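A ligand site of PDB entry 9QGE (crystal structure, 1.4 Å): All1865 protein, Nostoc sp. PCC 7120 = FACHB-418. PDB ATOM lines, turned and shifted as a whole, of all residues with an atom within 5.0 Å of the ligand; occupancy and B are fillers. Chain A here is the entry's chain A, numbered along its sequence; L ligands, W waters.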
ATOM      1  N   ALA A  35      -1.051 -26.431 -20.593  1.00  0.00           N
ATOM      2  CA  ALA A  35      -1.618 -26.223 -21.913  1.00  0.00           C
ATOM      3  C   ALA A  35      -2.653 -25.116 -21.859  1.00  0.00           C
ATOM      4  O   ALA A  35      -3.296 -24.877 -20.818  1.00  0.00           O
ATOM      5  CB  ALA A  35      -2.186 -27.534 -22.466  1.00  0.00           C
ATOM      6  N   PRO A  36      -2.867 -24.395 -22.985  1.00  0.00           N
ATOM      7  CA  PRO A  36      -3.951 -23.409 -23.048  1.00  0.00           C
ATOM      8  C   PRO A  36      -5.316 -24.053 -22.873  1.00  0.00           C
ATOM      9  O   PRO A  36      -5.644 -25.009 -23.563  1.00  0.00           O
ATOM     10  CB  PRO A  36      -3.786 -22.768 -24.448  1.00  0.00           C
ATOM     11  CG  PRO A  36      -3.079 -23.883 -25.243  1.00  0.00           C
ATOM     12  CD  PRO A  36      -2.111 -24.558 -24.258  1.00  0.00           C
ATOM     13  N   LEU A  37      -6.148 -23.460 -22.016  1.00  0.00           N
ATOM     14  CA  LEU A  37      -7.453 -24.029 -21.704  1.00  0.00           C
ATOM     15  C   LEU A  37      -8.510 -22.940 -21.602  1.00  0.00           C
ATOM     16  O   LEU A  37      -8.491 -22.164 -20.652  1.00  0.00           O
ATOM     17  CB  LEU A  37      -7.424 -24.812 -20.391  1.00  0.00           C
ATOM     18  CG  LEU A  37      -6.428 -25.978 -20.328  1.00  0.00           C
ATOM     19  CD1 LEU A  37      -5.953 -26.217 -18.856  1.00  0.00           C
ATOM     20  CD2 LEU A  37      -7.068 -27.222 -20.905  1.00  0.00           C
ATOM     21  N   THR A  38      -9.394 -22.924 -22.596  1.00  0.00           N
ATOM     22  CA  THR A  38     -10.574 -22.058 -22.599  1.00  0.00           C
ATOM     23  C   THR A  38     -11.446 -22.402 -21.393  1.00  0.00           C
ATOM     24  O   THR A  38     -11.877 -23.556 -21.269  1.00  0.00           O
ATOM     25  CB  THR A  38     -11.381 -22.274 -23.880  1.00  0.00           C
ATOM     26  OG1 THR A  38     -10.599 -21.714 -24.941  1.00  0.00           O
ATOM     27  CG2 THR A  38     -12.737 -21.562 -23.840  1.00  0.00           C
ATOM     28  N   ARG A  39     -11.742 -21.405 -20.529  1.00  0.00           N
ATOM     29  CA  ARG A  39     -12.583 -21.619 -19.351  1.00  0.00           C
ATOM     30  C   ARG A  39     -13.833 -20.731 -19.370  1.00  0.00           C
ATOM     31  O   ARG A  39     -14.706 -20.887 -18.496  1.00  0.00           O
ATOM     32  CB  ARG A  39     -11.760 -21.380 -18.078  1.00  0.00           C
ATOM     33  CG  ARG A  39     -10.516 -22.271 -17.949  1.00  0.00           C
ATOM     34  CD  ARG A  39     -10.648 -23.811 -18.142  1.00  0.00           C
ATOM     35  NE  ARG A  39     -11.637 -24.348 -17.200  1.00  0.00           N
ATOM     36  CZ  ARG A  39     -11.343 -24.648 -15.924  1.00  0.00           C
ATOM     37  NH1 ARG A  39     -10.099 -24.505 -15.471  1.00  0.00           N
ATOM     38  NH2 ARG A  39     -12.319 -25.075 -15.124  1.00  0.00           N
ATOM     39  N   GLU A  68      -5.231 -19.443 -21.650  1.00  0.00           N
ATOM     40  CA  GLU A  68      -6.351 -19.733 -22.527  1.00  0.00           C
ATOM     41  C   GLU A  68      -6.285 -18.923 -23.836  1.00  0.00           C
ATOM     42  O   GLU A  68      -5.855 -17.758 -23.851  1.00  0.00           O
ATOM     43  CB  GLU A  68      -7.649 -19.420 -21.788  1.00  0.00           C
ATOM     44  CG  GLU A  68      -7.910 -17.938 -21.483  1.00  0.00           C
ATOM     45  CD  GLU A  68      -8.731 -17.747 -20.221  1.00  0.00           C
ATOM     46  OE1 GLU A  68      -9.973 -17.795 -20.368  1.00  0.00           O
ATOM     47  OE2 GLU A  68      -8.154 -17.531 -19.141  1.00  0.00           O
ATOM     48  N   ALA A  69      -6.913 -19.493 -24.881  1.00  0.00           N
ATOM     49  CA  ALA A  69      -7.088 -18.760 -26.132  1.00  0.00           C
ATOM     50  C   ALA A  69      -7.827 -17.436 -25.889  1.00  0.00           C
ATOM     51  O   ALA A  69      -8.855 -17.376 -25.203  1.00  0.00           O
ATOM     52  CB  ALA A  69      -7.844 -19.646 -27.089  1.00  0.00           C
ATOM     53  N   GLN A 111      -2.027 -17.125 -25.230  1.00  0.00           N
ATOM     54  CA  GLN A 111      -2.376 -17.731 -26.530  1.00  0.00           C
ATOM     55  C   GLN A 111      -3.286 -16.773 -27.318  1.00  0.00           C
ATOM     56  O   GLN A 111      -4.347 -16.391 -26.840  1.00  0.00           O
ATOM     57  CB  GLN A 111      -3.047 -19.104 -26.406  1.00  0.00           C
ATOM     58  CG  GLN A 111      -3.105 -19.814 -27.760  1.00  0.00           C
ATOM     59  CD  GLN A 111      -3.904 -21.086 -27.765  1.00  0.00           C
ATOM     60  OE1 GLN A 111      -5.069 -21.116 -27.338  1.00  0.00           O
ATOM     61  NE2 GLN A 111      -3.277 -22.166 -28.222  1.00  0.00           N
ATOM     62  N   HIS A 187      -2.146 -19.317 -31.909  1.00  0.00           N
ATOM     63  CA  HIS A 187      -3.056 -20.455 -32.005  1.00  0.00           C
ATOM     64  C   HIS A 187      -3.259 -20.731 -33.493  1.00  0.00           C
ATOM     65  O   HIS A 187      -4.110 -20.102 -34.139  1.00  0.00           O
ATOM     66  CB  HIS A 187      -4.375 -20.151 -31.287  1.00  0.00           C
ATOM     67  CG  HIS A 187      -5.141 -21.416 -31.086  1.00  0.00           C
ATOM     68  ND1 HIS A 187      -6.215 -21.581 -30.242  1.00  0.00           N
ATOM     69  CD2 HIS A 187      -4.963 -22.575 -31.711  1.00  0.00           C
ATOM     70  CE1 HIS A 187      -6.685 -22.841 -30.363  1.00  0.00           C
ATOM     71  NE2 HIS A 187      -5.915 -23.461 -31.250  1.00  0.00           N
ATOM     72  N   ASN A 190      -6.586 -26.532 -33.982  1.00  0.00           N
ATOM     73  CA  ASN A 190      -7.967 -26.837 -33.599  1.00  0.00           C
ATOM     74  C   ASN A 190      -9.012 -26.236 -34.540  1.00  0.00           C
ATOM     75  O   ASN A 190     -10.170 -26.092 -34.161  1.00  0.00           O
ATOM     76  CB  ASN A 190      -8.226 -26.496 -32.133  1.00  0.00           C
ATOM     77  CG  ASN A 190      -7.314 -27.278 -31.212  1.00  0.00           C
ATOM     78  OD1 ASN A 190      -6.735 -28.305 -31.607  1.00  0.00           O
ATOM     79  ND2 ASN A 190      -7.150 -26.780 -29.987  1.00  0.00           N
ATOM     80  N   ARG A 239       1.365 -23.026 -32.101  1.00  0.00           N
ATOM     81  CA  ARG A 239       0.710 -24.306 -31.806  1.00  0.00           C
ATOM     82  C   ARG A 239       0.015 -24.836 -33.071  1.00  0.00           C
ATOM     83  O   ARG A 239      -0.728 -24.095 -33.724  1.00  0.00           O
ATOM     84  CB  ARG A 239      -0.316 -24.147 -30.681  1.00  0.00           C
ATOM     85  CG  ARG A 239      -0.743 -25.521 -30.153  1.00  0.00           C
ATOM     86  CD  ARG A 239      -1.714 -25.462 -28.942  1.00  0.00           C
ATOM     87  NE  ARG A 239      -1.485 -26.677 -28.164  1.00  0.00           N
ATOM     88  CZ  ARG A 239      -2.370 -27.210 -27.280  1.00  0.00           C
ATOM     89  NH1 ARG A 239      -3.633 -26.840 -27.282  1.00  0.00           N
ATOM     90  NH2 ARG A 239      -1.944 -28.091 -26.379  1.00  0.00           N
ATOM     91  N   PHE A 276      -0.215 -30.394 -30.409  1.00  0.00           N
ATOM     92  CA  PHE A 276      -1.310 -31.156 -29.770  1.00  0.00           C
ATOM     93  C   PHE A 276      -1.530 -32.389 -30.636  1.00  0.00           C
ATOM     94  O   PHE A 276      -1.912 -32.277 -31.825  1.00  0.00           O
ATOM     95  CB  PHE A 276      -2.517 -30.227 -29.689  1.00  0.00           C
ATOM     96  CG  PHE A 276      -3.841 -30.877 -29.341  1.00  0.00           C
ATOM     97  CD1 PHE A 276      -3.888 -32.122 -28.691  1.00  0.00           C
ATOM     98  CD2 PHE A 276      -5.047 -30.251 -29.691  1.00  0.00           C
ATOM     99  CE1 PHE A 276      -5.109 -32.721 -28.394  1.00  0.00           C
ATOM    100  CE2 PHE A 276      -6.258 -30.851 -29.364  1.00  0.00           C
ATOM    101  CZ  PHE A 276      -6.273 -32.087 -28.746  1.00  0.00           C
ATOM    102  N   ILE A 279      -5.978 -37.315 -29.648  1.00  0.00           N
ATOM    103  CA  ILE A 279      -6.085 -38.552 -28.891  1.00  0.00           C
ATOM    104  C   ILE A 279      -6.793 -39.636 -29.703  1.00  0.00           C
ATOM    105  O   ILE A 279      -6.586 -40.819 -29.406  1.00  0.00           O
ATOM    106  CB  ILE A 279      -6.767 -38.293 -27.524  1.00  0.00           C
ATOM    107  CG1 ILE A 279      -5.975 -37.238 -26.726  1.00  0.00           C
ATOM    108  CG2 ILE A 279      -7.060 -39.559 -26.715  1.00  0.00           C
ATOM    109  CD1 ILE A 279      -4.567 -37.631 -26.346  1.00  0.00           C
ATOM    110  N   ASN A 306       1.932 -32.653 -26.499  1.00  0.00           N
ATOM    111  CA  ASN A 306       0.741 -32.600 -25.677  1.00  0.00           C
ATOM    112  C   ASN A 306      -0.251 -33.642 -26.176  1.00  0.00           C
ATOM    113  O   ASN A 306      -0.295 -33.931 -27.375  1.00  0.00           O
ATOM    114  CB  ASN A 306       0.125 -31.207 -25.770  1.00  0.00           C
ATOM    115  CG  ASN A 306      -1.327 -31.205 -25.331  1.00  0.00           C
ATOM    116  OD1 ASN A 306      -2.220 -31.353 -26.184  1.00  0.00           O
ATOM    117  ND2 ASN A 306      -1.597 -31.160 -24.028  1.00  0.00           N
ATOM    118  N   GLY A 307      -1.021 -34.186 -25.227  1.00  0.00           N
ATOM    119  CA  GLY A 307      -2.174 -35.033 -25.506  1.00  0.00           C
ATOM    120  C   GLY A 307      -2.055 -36.346 -24.732  1.00  0.00           C
ATOM    121  O   GLY A 307      -1.333 -37.257 -25.125  1.00  0.00           O
ATOM    122  N   GLY A 308      -2.742 -36.397 -23.580  1.00  0.00           N
ATOM    123  CA  GLY A 308      -2.862 -37.637 -22.822  1.00  0.00           C
ATOM    124  C   GLY A 308      -1.572 -38.009 -22.079  1.00  0.00           C
ATOM    125  O   GLY A 308      -1.402 -39.157 -21.696  1.00  0.00           O
ATOM    126  N   TYR A 309      -0.691 -37.035 -21.836  1.00  0.00           N
ATOM    127  CA  TYR A 309       0.546 -37.332 -21.130  1.00  0.00           C
ATOM    128  C   TYR A 309       0.347 -37.624 -19.632  1.00  0.00           C
ATOM    129  O   TYR A 309      -0.621 -37.184 -19.000  1.00  0.00           O
ATOM    130  CB  TYR A 309       1.594 -36.245 -21.408  1.00  0.00           C
ATOM    131  CG  TYR A 309       2.221 -36.411 -22.790  1.00  0.00           C
ATOM    132  CD1 TYR A 309       1.628 -35.863 -23.930  1.00  0.00           C
ATOM    133  CD2 TYR A 309       3.337 -37.235 -22.972  1.00  0.00           C
ATOM    134  CE1 TYR A 309       2.162 -36.099 -25.192  1.00  0.00           C
ATOM    135  CE2 TYR A 309       3.865 -37.476 -24.222  1.00  0.00           C
ATOM    136  CZ  TYR A 309       3.277 -36.904 -25.335  1.00  0.00           C
ATOM    137  OH  TYR A 309       3.835 -37.145 -26.564  1.00  0.00           O
ATOM    138  N   ALA A 327       3.242 -30.535 -22.362  1.00  0.00           N
ATOM    139  CA  ALA A 327       2.118 -29.746 -21.852  1.00  0.00           C
ATOM    140  C   ALA A 327       0.975 -30.659 -21.414  1.00  0.00           C
ATOM    141  O   ALA A 327       0.621 -31.599 -22.109  1.00  0.00           O
ATOM    142  CB  ALA A 327       1.638 -28.701 -22.872  1.00  0.00           C
ATOM    143  N   PHE A 328       0.332 -30.279 -20.296  1.00  0.00           N
ATOM    144  CA  PHE A 328      -0.797 -31.006 -19.733  1.00  0.00           C
ATOM    145  C   PHE A 328      -1.992 -30.048 -19.701  1.00  0.00           C
ATOM    146  O   PHE A 328      -1.840 -28.924 -19.217  1.00  0.00           O
ATOM    147  CB  PHE A 328      -0.506 -31.416 -18.286  1.00  0.00           C
ATOM    148  CG  PHE A 328       0.663 -32.391 -18.205  1.00  0.00           C
ATOM    149  CD1 PHE A 328       1.974 -31.940 -18.230  1.00  0.00           C
ATOM    150  CD2 PHE A 328       0.446 -33.770 -18.017  1.00  0.00           C
ATOM    151  CE1 PHE A 328       3.035 -32.843 -18.172  1.00  0.00           C
ATOM    152  CE2 PHE A 328       1.501 -34.667 -17.919  1.00  0.00           C
ATOM    153  CZ  PHE A 328       2.799 -34.201 -17.985  1.00  0.00           C
ATOM    154  N   GLY A 329      -3.148 -30.484 -20.247  1.00  0.00           N
ATOM    155  CA  GLY A 329      -4.359 -29.672 -20.227  1.00  0.00           C
ATOM    156  C   GLY A 329      -5.263 -30.131 -19.086  1.00  0.00           C
ATOM    157  O   GLY A 329      -5.285 -29.508 -18.006  1.00  0.00           O
ATOM    158  N   THR A 330      -5.981 -31.235 -19.328  1.00  0.00           N
ATOM    159  CA  THR A 330      -6.975 -31.740 -18.377  1.00  0.00           C
ATOM    160  C   THR A 330      -6.430 -31.796 -16.946  1.00  0.00           C
ATOM    161  O   THR A 330      -7.108 -31.367 -15.997  1.00  0.00           O
ATOM    162  CB  THR A 330      -7.518 -33.084 -18.865  1.00  0.00           C
ATOM    163  OG1 THR A 330      -7.922 -32.950 -20.228  1.00  0.00           O
ATOM    164  CG2 THR A 330      -8.691 -33.551 -18.005  1.00  0.00           C
ATOM    165  N   ILE A 333      -6.378 -28.588 -15.108  1.00  0.00           N
ATOM    166  CA  ILE A 333      -7.687 -28.122 -14.628  1.00  0.00           C
ATOM    167  C   ILE A 333      -7.869 -28.550 -13.173  1.00  0.00           C
ATOM    168  O   ILE A 333      -8.208 -27.742 -12.317  1.00  0.00           O
ATOM    169  CB  ILE A 333      -8.854 -28.614 -15.512  1.00  0.00           C
ATOM    170  CG1 ILE A 333      -8.708 -28.029 -16.942  1.00  0.00           C
ATOM    171  CG2 ILE A 333     -10.225 -28.291 -14.869  1.00  0.00           C
ATOM    172  CD1 ILE A 333      -9.781 -28.450 -17.929  1.00  0.00           C
ATOM    173  N   PHE A 356     -15.927 -27.264 -16.767  1.00  0.00           N
ATOM    174  CA  PHE A 356     -14.847 -26.756 -17.613  1.00  0.00           C
ATOM    175  C   PHE A 356     -15.133 -25.347 -18.107  1.00  0.00           C
ATOM    176  O   PHE A 356     -14.239 -24.480 -18.095  1.00  0.00           O
ATOM    177  CB  PHE A 356     -14.531 -27.697 -18.784  1.00  0.00           C
ATOM    178  CG  PHE A 356     -13.844 -29.003 -18.445  1.00  0.00           C
ATOM    179  CD1 PHE A 356     -13.426 -29.259 -17.138  1.00  0.00           C
ATOM    180  CD2 PHE A 356     -13.528 -29.920 -19.443  1.00  0.00           C
ATOM    181  CE1 PHE A 356     -12.797 -30.457 -16.827  1.00  0.00           C
ATOM    182  CE2 PHE A 356     -12.878 -31.119 -19.140  1.00  0.00           C
ATOM    183  CZ  PHE A 356     -12.516 -31.386 -17.829  1.00  0.00           C
ATOM    184  N   TYR A 357     -16.364 -25.122 -18.600  1.00  0.00           N
ATOM    185  CA  TYR A 357     -16.639 -23.870 -19.303  1.00  0.00           C
ATOM    186  C   TYR A 357     -17.729 -23.074 -18.587  1.00  0.00           C
ATOM    187  O   TYR A 357     -18.758 -23.635 -18.221  1.00  0.00           O
ATOM    188  CB  TYR A 357     -17.151 -24.161 -20.716  1.00  0.00           C
ATOM    189  CG  TYR A 357     -16.203 -24.981 -21.563  1.00  0.00           C
ATOM    190  CD1 TYR A 357     -15.103 -24.374 -22.151  1.00  0.00           C
ATOM    191  CD2 TYR A 357     -16.445 -26.320 -21.864  1.00  0.00           C
ATOM    192  CE1 TYR A 357     -14.238 -25.086 -22.954  1.00  0.00           C
ATOM    193  CE2 TYR A 357     -15.576 -27.048 -22.655  1.00  0.00           C
ATOM    194  CZ  TYR A 357     -14.464 -26.419 -23.205  1.00  0.00           C
ATOM    195  OH  TYR A 357     -13.634 -27.108 -24.049  1.00  0.00           O
HETATM  196  N1  LIG L   1      -6.364 -25.873 -26.871  1.00  0.00           N
HETATM  197  C1  LIG L   1      -5.943 -24.651 -27.278  1.00  0.00           C
HETATM  198  O1  LIG L   1      -5.009 -24.582 -28.131  1.00  0.00           O
HETATM  199  N2  LIG L   1      -6.508 -23.478 -26.790  1.00  0.00           N
HETATM  200  C2  LIG L   1      -7.524 -23.505 -25.860  1.00  0.00           C
HETATM  201  O2  LIG L   1      -7.985 -22.438 -25.422  1.00  0.00           O
HETATM  202  C3  LIG L   1      -8.007 -24.780 -25.453  1.00  0.00           C
HETATM  203  N3  LIG L   1      -9.039 -24.833 -24.613  1.00  0.00           N
HETATM  204  C4  LIG L   1      -9.328 -26.066 -24.085  1.00  0.00           C
HETATM  205  C5  LIG L   1     -10.333 -26.128 -23.090  1.00  0.00           C
HETATM  206  C6  LIG L   1     -10.632 -27.312 -22.466  1.00  0.00           C
HETATM  207  C7  LIG L   1     -11.656 -27.311 -21.342  1.00  0.00           C
HETATM  208  C8  LIG L   1      -9.991 -28.511 -22.864  1.00  0.00           C
HETATM  209  C9  LIG L   1     -10.326 -29.827 -22.182  1.00  0.00           C
HETATM  210  C10 LIG L   1      -9.091 -28.486 -23.920  1.00  0.00           C
HETATM  211  C11 LIG L   1      -8.712 -27.259 -24.516  1.00  0.00           C
HETATM  212  N4  LIG L   1      -7.741 -27.171 -25.517  1.00  0.00           N
HETATM  213  C12 LIG L   1      -7.309 -25.940 -25.948  1.00  0.00           C
HETATM  214  C13 LIG L   1      -6.941 -28.351 -25.860  1.00  0.00           C
HETATM  215  C14 LIG L   1      -5.889 -28.555 -24.729  1.00  0.00           C
HETATM  216  O3  LIG L   1      -4.940 -27.468 -24.642  1.00  0.00           O
HETATM  217  C15 LIG L   1      -5.081 -29.843 -24.821  1.00  0.00           C
HETATM  218  O4  LIG L   1      -4.392 -29.763 -26.067  1.00  0.00           O
HETATM  219  C16 LIG L   1      -5.952 -31.094 -24.858  1.00  0.00           C
HETATM  220  O5  LIG L   1      -6.882 -31.070 -23.781  1.00  0.00           O
HETATM  221  C17 LIG L   1      -5.111 -32.359 -24.820  1.00  0.00           C
HETATM  222  O6  LIG L   1      -4.172 -32.399 -23.712  1.00  0.00           O
HETATM  223  P1  LIG L   1      -4.571 -33.188 -22.341  1.00  0.00           P
HETATM  224  O7  LIG L   1      -5.807 -32.544 -21.780  1.00  0.00           O
HETATM  225  O8  LIG L   1      -4.794 -34.626 -22.752  1.00  0.00           O
HETATM  226  O9  LIG L   1      -3.333 -32.982 -21.458  1.00  0.00           O
HETATM  227  O   HOH W   1      -0.922 -33.980 -22.337  1.00  0.00           O
HETATM  228  O   HOH W   2      -9.050 -32.195 -25.065  1.00  0.00           O
HETATM  229  O   HOH W   3      -5.304 -36.482 -20.735  1.00  0.00           O
HETATM  230  O   HOH W   4      -3.520 -33.672 -18.766  1.00  0.00           O
HETATM  231  O   HOH W   5      -7.037 -35.623 -23.811  1.00  0.00           O
HETATM  232  O   HOH W   6     -11.346 -32.562 -23.843  1.00  0.00           O
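Residues that only touch the ligand: Tyr 357 (3.4 Å), Leu 37 (3.4 Å), Phe 276 (3.5 Å), Ala 35 (3.5 Å), Phe 328 (3.6 Å), Phe 356 (3.7 Å) and Gly 307 (3.8 Å).
Hydrophobic or aromatic side chains that line the ligand: Ala 35, Pro 36, Leu 37, Ala 69, His 187, Phe 276, Phe 356 and Tyr 357.
Within 4 Å of the ligand: Ala 35, Pro 36, Leu 37, Thr 38, Ala 69, Gln 111, His 187, Asn 190, Arg 239, Phe 276, Asn 306, Gly 307, Gly 308, Phe 328, Gly 329, Thr 330, Phe 356 and Tyr 357.
The nearest printed residue that does not touch the ligand is Ile 333 (4.1 Å).
N of Thr 330 sits at hydrogen-bond distance from O7 of the ligand, at 2.8 Å.
An oxygen (O7) of the ligand sits at hydrogen-bond distance from the side-chain hydroxyl (OG1) of Thr 330 (2.7 Å).
An oxygen (O4) of the ligand sits at hydrogen-bond distance from the side-chain amide oxygen (OD1) of Asn 306, at 2.7 Å.
N of Thr 38 lies within hydrogen-bond range of N3 of the ligand (2.8 Å).
The side-chain hydroxyl of Thr 38 is in hydrogen-bond range of an oxygen (O2) of the ligand (2.8 Å).
O3 of the ligand lies within hydrogen-bond range of O of Pro 36, 2.8 Å away.
The guanidinium group (NH1) of Arg 239 is in hydrogen-bond range of an oxygen (O1) of the ligand (2.8 Å).
The backbone NH of Gly 329 lies within hydrogen-bond range of an oxygen (O9) of the ligand.
OE1 of Gln 111 lies within hydrogen-bond range of N2 of the ligand, 2.8 Å away.
An oxygen (O8) of the ligand sits at hydrogen-bond distance from the backbone NH (N) of Gly 308, at 2.8 Å.
O2 of the ligand sits at hydrogen-bond distance from N of Ala 69 (3.2 Å).
NE2 of His 187 sits close to O1 of the ligand.
The side-chain amide nitrogen (ND2) of Asn 190 sits at hydrogen-bond distance from a nitrogen (N1) of the ligand (3.3 Å).
NH2 of Arg 239 is in hydrogen-bond range of OD1 of Asn 306, 3.3 Å away.
The side-chain amide nitrogen (ND2) of Asn 306 sits at hydrogen-bond distance from the backbone carbonyl oxygen (O) of Ala 327 (3.0 Å).
OE1 of Gln 111 lies close to N of Ala 69, at 3.5 Å.
ND1 of His 187 lies within hydrogen-bond range of OE1 of Gln 111 (3.2 Å).
The backbone carbonyl oxygen (O) of Phe 328 lies within hydrogen-bond range of the backbone NH (N) of Ala 35 (3.0 Å).
The backbone carbonyl oxygen (O) of Phe 356 sits at hydrogen-bond distance from the guanidinium group (NE) of Arg 39 (2.8 Å).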
